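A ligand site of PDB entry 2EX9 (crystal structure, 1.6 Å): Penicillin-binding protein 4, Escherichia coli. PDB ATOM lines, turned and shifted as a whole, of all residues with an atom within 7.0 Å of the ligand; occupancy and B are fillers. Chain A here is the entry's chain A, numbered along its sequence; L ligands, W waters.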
ATOM      1  N   PRO A  41      26.826 -10.593   2.367  1.00  0.00           N
ATOM      2  CA  PRO A  41      26.186  -9.462   1.716  1.00  0.00           C
ATOM      3  C   PRO A  41      25.402  -8.555   2.674  1.00  0.00           C
ATOM      4  O   PRO A  41      25.101  -7.405   2.346  1.00  0.00           O
ATOM      5  CB  PRO A  41      25.282 -10.136   0.671  1.00  0.00           C
ATOM      6  CG  PRO A  41      24.826 -11.463   1.297  1.00  0.00           C
ATOM      7  CD  PRO A  41      26.099 -11.850   2.117  1.00  0.00           C
ATOM      8  N   ALA A  42      25.029  -9.080   3.835  1.00  0.00           N
ATOM      9  CA  ALA A  42      24.166  -8.328   4.757  1.00  0.00           C
ATOM     10  C   ALA A  42      22.954  -7.824   3.970  1.00  0.00           C
ATOM     11  O   ALA A  42      22.508  -8.504   3.092  1.00  0.00           O
ATOM     12  CB  ALA A  42      24.942  -7.206   5.475  1.00  0.00           C
ATOM     13  N   SER A  43      22.405  -6.655   4.284  1.00  0.00           N
ATOM     14  CA  SER A  43      21.148  -6.206   3.630  1.00  0.00           C
ATOM     15  C   SER A  43      21.209  -5.935   2.101  1.00  0.00           C
ATOM     16  O   SER A  43      20.178  -5.661   1.495  1.00  0.00           O
ATOM     17  CB  SER A  43      20.616  -4.971   4.363  1.00  0.00           C
ATOM     18  OG  SER A  43      19.905  -5.392   5.529  1.00  0.00           O
ATOM     19  N   THR A  44      22.378  -6.044   1.459  1.00  0.00           N
ATOM     20  CA  THR A  44      22.364  -5.925  -0.005  1.00  0.00           C
ATOM     21  C   THR A  44      21.653  -7.119  -0.635  1.00  0.00           C
ATOM     22  O   THR A  44      21.282  -7.089  -1.811  1.00  0.00           O
ATOM     23  CB  THR A  44      23.783  -5.745  -0.631  1.00  0.00           C
ATOM     24  OG1 THR A  44      24.530  -6.931  -0.390  1.00  0.00           O
ATOM     25  CG2 THR A  44      24.563  -4.590   0.059  1.00  0.00           C
ATOM     26  N   LYS A  46      18.773  -7.816  -0.190  1.00  0.00           N
ATOM     27  CA  LYS A  46      17.452  -7.267  -0.526  1.00  0.00           C
ATOM     28  C   LYS A  46      17.322  -6.872  -2.008  1.00  0.00           C
ATOM     29  O   LYS A  46      16.228  -6.980  -2.586  1.00  0.00           O
ATOM     30  CB  LYS A  46      17.119  -6.107   0.405  1.00  0.00           C
ATOM     31  CG  LYS A  46      16.769  -6.555   1.855  1.00  0.00           C
ATOM     32  CD  LYS A  46      16.244  -5.381   2.618  1.00  0.00           C
ATOM     33  CE  LYS A  46      15.946  -5.821   4.056  1.00  0.00           C
ATOM     34  NZ  LYS A  46      17.192  -5.751   4.908  1.00  0.00           N
ATOM     35  N   ASP A 136      19.671 -12.190  18.953  1.00  0.00           N
ATOM     36  CA  ASP A 136      18.962 -11.017  18.434  1.00  0.00           C
ATOM     37  C   ASP A 136      17.483 -11.339  18.197  1.00  0.00           C
ATOM     38  O   ASP A 136      16.722 -10.458  17.782  1.00  0.00           O
ATOM     39  CB  ASP A 136      19.601 -10.571  17.127  1.00  0.00           C
ATOM     40  CG  ASP A 136      20.943  -9.937  17.325  1.00  0.00           C
ATOM     41  OD1 ASP A 136      21.126  -9.199  18.318  1.00  0.00           O
ATOM     42  OD2 ASP A 136      21.872 -10.102  16.505  1.00  0.00           O
ATOM     43  N   PHE A 141      14.203  -5.898  15.033  1.00  0.00           N
ATOM     44  CA  PHE A 141      14.764  -6.000  13.686  1.00  0.00           C
ATOM     45  C   PHE A 141      14.897  -7.445  13.231  1.00  0.00           C
ATOM     46  O   PHE A 141      14.986  -7.741  12.040  1.00  0.00           O
ATOM     47  CB  PHE A 141      16.121  -5.282  13.535  1.00  0.00           C
ATOM     48  CG  PHE A 141      17.281  -5.965  14.237  1.00  0.00           C
ATOM     49  CD1 PHE A 141      17.992  -6.987  13.588  1.00  0.00           C
ATOM     50  CD2 PHE A 141      17.692  -5.534  15.485  1.00  0.00           C
ATOM     51  CE1 PHE A 141      19.079  -7.613  14.220  1.00  0.00           C
ATOM     52  CE2 PHE A 141      18.759  -6.166  16.125  1.00  0.00           C
ATOM     53  CZ  PHE A 141      19.459  -7.182  15.464  1.00  0.00           C
ATOM     54  N   SER A 142      14.874  -8.359  14.197  1.00  0.00           N
ATOM     55  CA  SER A 142      14.994  -9.784  13.913  1.00  0.00           C
ATOM     56  C   SER A 142      13.701 -10.518  14.305  1.00  0.00           C
ATOM     57  O   SER A 142      13.696 -11.757  14.464  1.00  0.00           O
ATOM     58  CB  SER A 142      16.198 -10.345  14.676  1.00  0.00           C
ATOM     59  OG  SER A 142      16.407 -11.719  14.326  1.00  0.00           O
ATOM     60  N   LYS A 286      14.245   1.698   3.277  1.00  0.00           N
ATOM     61  CA  LYS A 286      14.426   1.628   4.727  1.00  0.00           C
ATOM     62  C   LYS A 286      15.178   0.384   5.199  1.00  0.00           C
ATOM     63  O   LYS A 286      15.490   0.270   6.393  1.00  0.00           O
ATOM     64  CB  LYS A 286      13.050   1.643   5.396  1.00  0.00           C
ATOM     65  CG  LYS A 286      12.392   3.012   5.337  1.00  0.00           C
ATOM     66  CD  LYS A 286      11.192   3.104   6.277  1.00  0.00           C
ATOM     67  CE  LYS A 286      10.442   4.459   6.083  1.00  0.00           C
ATOM     68  NZ  LYS A 286      11.307   5.619   6.563  1.00  0.00           N
ATOM     69  N   SER A 287      15.429  -0.551   4.283  1.00  0.00           N
ATOM     70  CA  SER A 287      16.058  -1.862   4.593  1.00  0.00           C
ATOM     71  C   SER A 287      15.188  -2.671   5.530  1.00  0.00           C
ATOM     72  O   SER A 287      15.666  -3.131   6.585  1.00  0.00           O
ATOM     73  CB  SER A 287      17.467  -1.749   5.197  1.00  0.00           C
ATOM     74  OG  SER A 287      18.184  -2.955   4.856  1.00  0.00           O
ATOM     75  N   ASP A 288      13.926  -2.845   5.147  1.00  0.00           N
ATOM     76  CA  ASP A 288      12.903  -3.455   5.998  1.00  0.00           C
ATOM     77  C   ASP A 288      13.025  -4.961   5.954  1.00  0.00           C
ATOM     78  O   ASP A 288      12.582  -5.630   5.027  1.00  0.00           O
ATOM     79  CB  ASP A 288      11.506  -2.956   5.578  1.00  0.00           C
ATOM     80  CG  ASP A 288      10.451  -3.299   6.575  1.00  0.00           C
ATOM     81  OD1 ASP A 288      10.441  -4.439   7.081  1.00  0.00           O
ATOM     82  OD2 ASP A 288       9.550  -2.508   6.906  1.00  0.00           O
ATOM     83  N   ASN A 289      13.669  -5.512   6.980  1.00  0.00           N
ATOM     84  CA  ASN A 289      13.845  -6.954   7.057  1.00  0.00           C
ATOM     85  C   ASN A 289      12.543  -7.752   6.971  1.00  0.00           C
ATOM     86  O   ASN A 289      12.494  -8.839   6.390  1.00  0.00           O
ATOM     87  CB  ASN A 289      14.544  -7.333   8.370  1.00  0.00           C
ATOM     88  CG  ASN A 289      15.975  -6.849   8.474  1.00  0.00           C
ATOM     89  OD1 ASN A 289      16.659  -6.488   7.484  1.00  0.00           O
ATOM     90  ND2 ASN A 289      16.482  -6.831   9.702  1.00  0.00           N
ATOM     91  N   SER A 338      16.236 -10.920   3.670  1.00  0.00           N
ATOM     92  CA  SER A 338      16.642  -9.654   4.299  1.00  0.00           C
ATOM     93  C   SER A 338      18.171  -9.371   4.309  1.00  0.00           C
ATOM     94  O   SER A 338      18.607  -8.209   4.444  1.00  0.00           O
ATOM     95  CB  SER A 338      16.153  -9.589   5.756  1.00  0.00           C
ATOM     96  OG  SER A 338      16.629 -10.757   6.443  1.00  0.00           O
ATOM     97  N   GLY A 339      18.968 -10.449   4.257  1.00  0.00           N
ATOM     98  CA  GLY A 339      20.421 -10.381   4.412  1.00  0.00           C
ATOM     99  C   GLY A 339      20.869 -10.539   5.867  1.00  0.00           C
ATOM    100  O   GLY A 339      22.056 -10.455   6.175  1.00  0.00           O
ATOM    101  N   LEU A 340      19.913 -10.785   6.760  1.00  0.00           N
ATOM    102  CA  LEU A 340      20.231 -10.957   8.186  1.00  0.00           C
ATOM    103  C   LEU A 340      21.103 -12.194   8.423  1.00  0.00           C
ATOM    104  O   LEU A 340      22.025 -12.174   9.266  1.00  0.00           O
ATOM    105  CB  LEU A 340      18.900 -11.061   8.969  1.00  0.00           C
ATOM    106  CG  LEU A 340      18.880 -11.106  10.481  1.00  0.00           C
ATOM    107  CD1 LEU A 340      19.754 -10.014  11.122  1.00  0.00           C
ATOM    108  CD2 LEU A 340      17.420 -10.953  10.961  1.00  0.00           C
ATOM    109  N   ARG A 342      23.844 -14.990   8.677  1.00  0.00           N
ATOM    110  CA  ARG A 342      25.309 -15.082   8.503  1.00  0.00           C
ATOM    111  C   ARG A 342      25.699 -16.212   7.551  1.00  0.00           C
ATOM    112  O   ARG A 342      26.887 -16.404   7.253  1.00  0.00           O
ATOM    113  CB  ARG A 342      26.036 -15.228   9.859  1.00  0.00           C
ATOM    114  CG  ARG A 342      25.781 -14.092  10.892  1.00  0.00           C
ATOM    115  CD  ARG A 342      25.506 -12.671  10.334  1.00  0.00           C
ATOM    116  NE  ARG A 342      25.607 -11.685  11.424  1.00  0.00           N
ATOM    117  CZ  ARG A 342      24.592 -11.118  12.095  1.00  0.00           C
ATOM    118  NH1 ARG A 342      23.299 -11.365  11.806  1.00  0.00           N
ATOM    119  NH2 ARG A 342      24.903 -10.240  13.050  1.00  0.00           N
ATOM    120  N   SER A 379      18.267   4.980   3.462  1.00  0.00           N
ATOM    121  CA  SER A 379      19.477   4.739   4.218  1.00  0.00           C
ATOM    122  C   SER A 379      20.623   5.665   3.851  1.00  0.00           C
ATOM    123  O   SER A 379      21.566   5.777   4.619  1.00  0.00           O
ATOM    124  CB  SER A 379      19.914   3.279   4.039  1.00  0.00           C
ATOM    125  OG  SER A 379      18.767   2.431   4.105  1.00  0.00           O
ATOM    126  N   LYS A 398      21.997   0.224  -2.355  1.00  0.00           N
ATOM    127  CA  LYS A 398      21.476  -0.459  -1.190  1.00  0.00           C
ATOM    128  C   LYS A 398      22.600  -0.672  -0.164  1.00  0.00           C
ATOM    129  O   LYS A 398      23.702  -1.108  -0.523  1.00  0.00           O
ATOM    130  CB  LYS A 398      20.924  -1.805  -1.611  1.00  0.00           C
ATOM    131  CG  LYS A 398      20.220  -2.585  -0.497  1.00  0.00           C
ATOM    132  CD  LYS A 398      18.971  -1.848   0.054  1.00  0.00           C
ATOM    133  CE  LYS A 398      18.462  -2.578   1.309  1.00  0.00           C
ATOM    134  NZ  LYS A 398      19.231  -2.192   2.497  1.00  0.00           N
ATOM    135  N   THR A 399      22.337  -0.341   1.094  1.00  0.00           N
ATOM    136  CA  THR A 399      23.335  -0.566   2.142  1.00  0.00           C
ATOM    137  C   THR A 399      23.219  -1.997   2.682  1.00  0.00           C
ATOM    138  O   THR A 399      22.234  -2.675   2.495  1.00  0.00           O
ATOM    139  CB  THR A 399      23.156   0.377   3.331  1.00  0.00           C
ATOM    140  OG1 THR A 399      21.803   0.281   3.828  1.00  0.00           O
ATOM    141  CG2 THR A 399      23.265   1.819   2.942  1.00  0.00           C
ATOM    142  N   GLY A 400      24.257  -2.426   3.385  1.00  0.00           N
ATOM    143  CA  GLY A 400      24.259  -3.728   4.049  1.00  0.00           C
ATOM    144  C   GLY A 400      25.095  -3.499   5.301  1.00  0.00           C
ATOM    145  O   GLY A 400      26.298  -3.311   5.211  1.00  0.00           O
ATOM    146  N   SER A 401      24.441  -3.507   6.469  1.00  0.00           N
ATOM    147  CA  SER A 401      25.123  -3.182   7.733  1.00  0.00           C
ATOM    148  C   SER A 401      24.877  -4.280   8.762  1.00  0.00           C
ATOM    149  O   SER A 401      23.729  -4.593   9.058  1.00  0.00           O
ATOM    150  CB  SER A 401      24.626  -1.842   8.283  1.00  0.00           C
ATOM    151  OG  SER A 401      24.481  -0.872   7.233  1.00  0.00           O
ATOM    152  N   LEU A 402      25.964  -4.854   9.275  1.00  0.00           N
ATOM    153  CA  LEU A 402      25.922  -5.847  10.337  1.00  0.00           C
ATOM    154  C   LEU A 402      27.182  -5.560  11.158  1.00  0.00           C
ATOM    155  O   LEU A 402      28.005  -4.705  10.751  1.00  0.00           O
ATOM    156  CB  LEU A 402      25.959  -7.275   9.777  1.00  0.00           C
ATOM    157  CG  LEU A 402      24.783  -7.913   9.007  1.00  0.00           C
ATOM    158  CD1 LEU A 402      25.136  -9.312   8.555  1.00  0.00           C
ATOM    159  CD2 LEU A 402      23.547  -7.961   9.876  1.00  0.00           C
ATOM    160  N   GLN A 403      27.320  -6.224  12.308  1.00  0.00           N
ATOM    161  CA  GLN A 403      28.484  -5.969  13.195  1.00  0.00           C
ATOM    162  C   GLN A 403      29.737  -6.073  12.353  1.00  0.00           C
ATOM    163  O   GLN A 403      30.067  -7.153  11.868  1.00  0.00           O
ATOM    164  CB  GLN A 403      28.506  -7.002  14.345  1.00  0.00           C
ATOM    165  CG  GLN A 403      29.704  -6.936  15.301  1.00  0.00           C
ATOM    166  CD  GLN A 403      29.608  -7.990  16.434  1.00  0.00           C
ATOM    167  OE1 GLN A 403      30.574  -8.738  16.681  1.00  0.00           O
ATOM    168  NE2 GLN A 403      28.453  -8.034  17.123  1.00  0.00           N
ATOM    169  N   GLY A 404      30.387  -4.927  12.123  1.00  0.00           N
ATOM    170  CA  GLY A 404      31.630  -4.853  11.357  1.00  0.00           C
ATOM    171  C   GLY A 404      31.489  -5.192   9.889  1.00  0.00           C
ATOM    172  O   GLY A 404      32.419  -5.724   9.268  1.00  0.00           O
ATOM    173  N   VAL A 405      30.315  -4.925   9.322  1.00  0.00           N
ATOM    174  CA  VAL A 405      30.094  -5.112   7.888  1.00  0.00           C
ATOM    175  C   VAL A 405      29.532  -3.813   7.375  1.00  0.00           C
ATOM    176  O   VAL A 405      28.538  -3.315   7.934  1.00  0.00           O
ATOM    177  CB  VAL A 405      29.132  -6.261   7.586  1.00  0.00           C
ATOM    178  CG1 VAL A 405      28.848  -6.333   6.086  1.00  0.00           C
ATOM    179  CG2 VAL A 405      29.708  -7.577   8.040  1.00  0.00           C
ATOM    180  N   TYR A 406      30.150  -3.242   6.332  1.00  0.00           N
ATOM    181  CA  TYR A 406      29.681  -1.986   5.741  1.00  0.00           C
ATOM    182  C   TYR A 406      29.635  -2.091   4.234  1.00  0.00           C
ATOM    183  O   TYR A 406      30.560  -1.672   3.554  1.00  0.00           O
ATOM    184  CB  TYR A 406      30.606  -0.828   6.118  1.00  0.00           C
ATOM    185  CG  TYR A 406      30.538  -0.446   7.587  1.00  0.00           C
ATOM    186  CD1 TYR A 406      29.384   0.154   8.117  1.00  0.00           C
ATOM    187  CD2 TYR A 406      31.605  -0.692   8.443  1.00  0.00           C
ATOM    188  CE1 TYR A 406      29.318   0.515   9.485  1.00  0.00           C
ATOM    189  CE2 TYR A 406      31.551  -0.349   9.781  1.00  0.00           C
ATOM    190  CZ  TYR A 406      30.409   0.255  10.293  1.00  0.00           C
ATOM    191  OH  TYR A 406      30.364   0.601  11.633  1.00  0.00           O
HETATM  192  C1  LIG L   1      23.852  -3.278  12.185  1.00  0.00           C
HETATM  193  C2  LIG L   1      24.931  -3.117  13.067  1.00  0.00           C
HETATM  194  C3  LIG L   1      25.108  -4.002  14.134  1.00  0.00           C
HETATM  195  C4  LIG L   1      24.212  -5.066  14.310  1.00  0.00           C
HETATM  196  C5  LIG L   1      23.145  -5.233  13.431  1.00  0.00           C
HETATM  197  C6  LIG L   1      22.955  -4.343  12.372  1.00  0.00           C
HETATM  198  O1  LIG L   1      21.922  -4.509  11.477  1.00  0.00           O
HETATM  199  C7  LIG L   1      21.177  -5.702  11.529  1.00  0.00           C
HETATM  200  C8  LIG L   1      20.330  -5.767  10.250  1.00  0.00           C
HETATM  201  O2  LIG L   1      19.290  -6.428  10.308  1.00  0.00           O
HETATM  202  N1  LIG L   1      20.734  -5.157   9.117  1.00  0.00           N
HETATM  203  C9  LIG L   1      19.883  -5.221   7.928  1.00  0.00           C
HETATM  204  C10 LIG L   1      20.708  -5.313   6.650  1.00  0.00           C
HETATM  205  O3  LIG L   1      21.928  -5.224   6.670  1.00  0.00           O
HETATM  206  C11 LIG L   1      19.041  -3.938   7.870  1.00  0.00           C
HETATM  207  N2  LIG L   1      19.847  -2.737   7.614  1.00  0.00           N
HETATM  208  S1  LIG L   1      18.171  -3.603   9.433  1.00  0.00           S
HETATM  209  C12 LIG L   1      18.788  -2.001   9.811  1.00  0.00           C
HETATM  210  C13 LIG L   1      17.684  -0.996   9.461  1.00  0.00           C
HETATM  211  C14 LIG L   1      19.119  -1.923  11.338  1.00  0.00           C
HETATM  212  C15 LIG L   1      20.023  -1.996   8.909  1.00  0.00           C
HETATM  213  C16 LIG L   1      20.439  -0.561   8.696  1.00  0.00           C
HETATM  214  O4  LIG L   1      20.053  -0.025   7.637  1.00  0.00           O
HETATM  215  O5  LIG L   1      21.091  -0.040   9.648  1.00  0.00           O
HETATM  216  O   HOH W   1      18.334   1.870   6.874  1.00  0.00           O
HETATM  217  O   HOH W   2      22.040   1.497   6.250  1.00  0.00           O
HETATM  218  O   HOH W   3      21.774  -1.936   5.577  1.00  0.00           O
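The backbone NH (N) of Ser 43 sits close to an oxygen (O3) of the ligand, at 2.8 Å.
OG of Ser 43 is covalently linked to C10 of the ligand (1.4 Å).
The side-chain amide nitrogen (ND2) of Asn 289 lies within hydrogen-bond range of an oxygen (O2) of the ligand (2.9 Å).
N of Ser 401 is in hydrogen-bond range of O3 of the ligand, 3.1 Å away.
The backbone carbonyl oxygen (O) of Ser 401 lies within hydrogen-bond range of a nitrogen (N1) of the ligand (3.0 Å).
The side-chain hydroxyl of Ser 287 is in hydrogen-bond range of a nitrogen (N2) of the ligand (3.2 Å).
OG of Ser 43 is in hydrogen-bond range of OG of Ser 287 (3.1 Å).
OG of Ser 43 lies within hydrogen-bond range of NZ of Lys 46, 2.8 Å away.
The side-chain amide nitrogen (ND2) of Asn 289 lies within hydrogen-bond range of the backbone carbonyl oxygen (O) of Phe 141 (2.9 Å).
The side-chain amide oxygen (OD1) of Asn 289 sits at hydrogen-bond distance from the side-chain amino group (NZ) of Lys 46, at 2.7 Å.
The side-chain amino group of Lys 46 lies within hydrogen-bond range of the side-chain hydroxyl of Ser 287, 3.0 Å away.
OG of Ser 338 is in hydrogen-bond range of N of Leu 340.
NH1 of Arg 342 is in hydrogen-bond range of O of Leu 340 (3.0 Å).
The side-chain amino group of Lys 46 sits at hydrogen-bond distance from the backbone carbonyl oxygen of Ser 338, at 2.9 Å.
Residues that only touch the ligand: Ala 42, Lys 46, Phe 141, Lys 286, Leu 340, Gly 400, Leu 402 and Gln 403.
Hydrophobic or aromatic side chains that line the ligand: Ala 42, Phe 141, Leu 340 and Leu 402.
12 residues have an atom within 4 Å of the ligand: Ala 42, Ser 43, Lys 46, Phe 141, Lys 286, Ser 287, Asn 289, Leu 340, Gly 400, Ser 401, Leu 402 and Gln 403.
The nearest printed residue that does not touch the ligand is Thr 399 (4.2 Å).
Water W1 lies within hydrogen-bond range of O4 of the ligand (2.7 Å), OG of Ser 379 (2.9 Å) and O of Lys 286 (3.3 Å).
Water W2 lies within hydrogen-bond range of OG1 of Thr 399 and O4 of the ligand.
Water W3 lies within hydrogen-bond range of OG1 of Thr 399, N2 of the ligand, N of Ser 401 and N of Gly 400.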
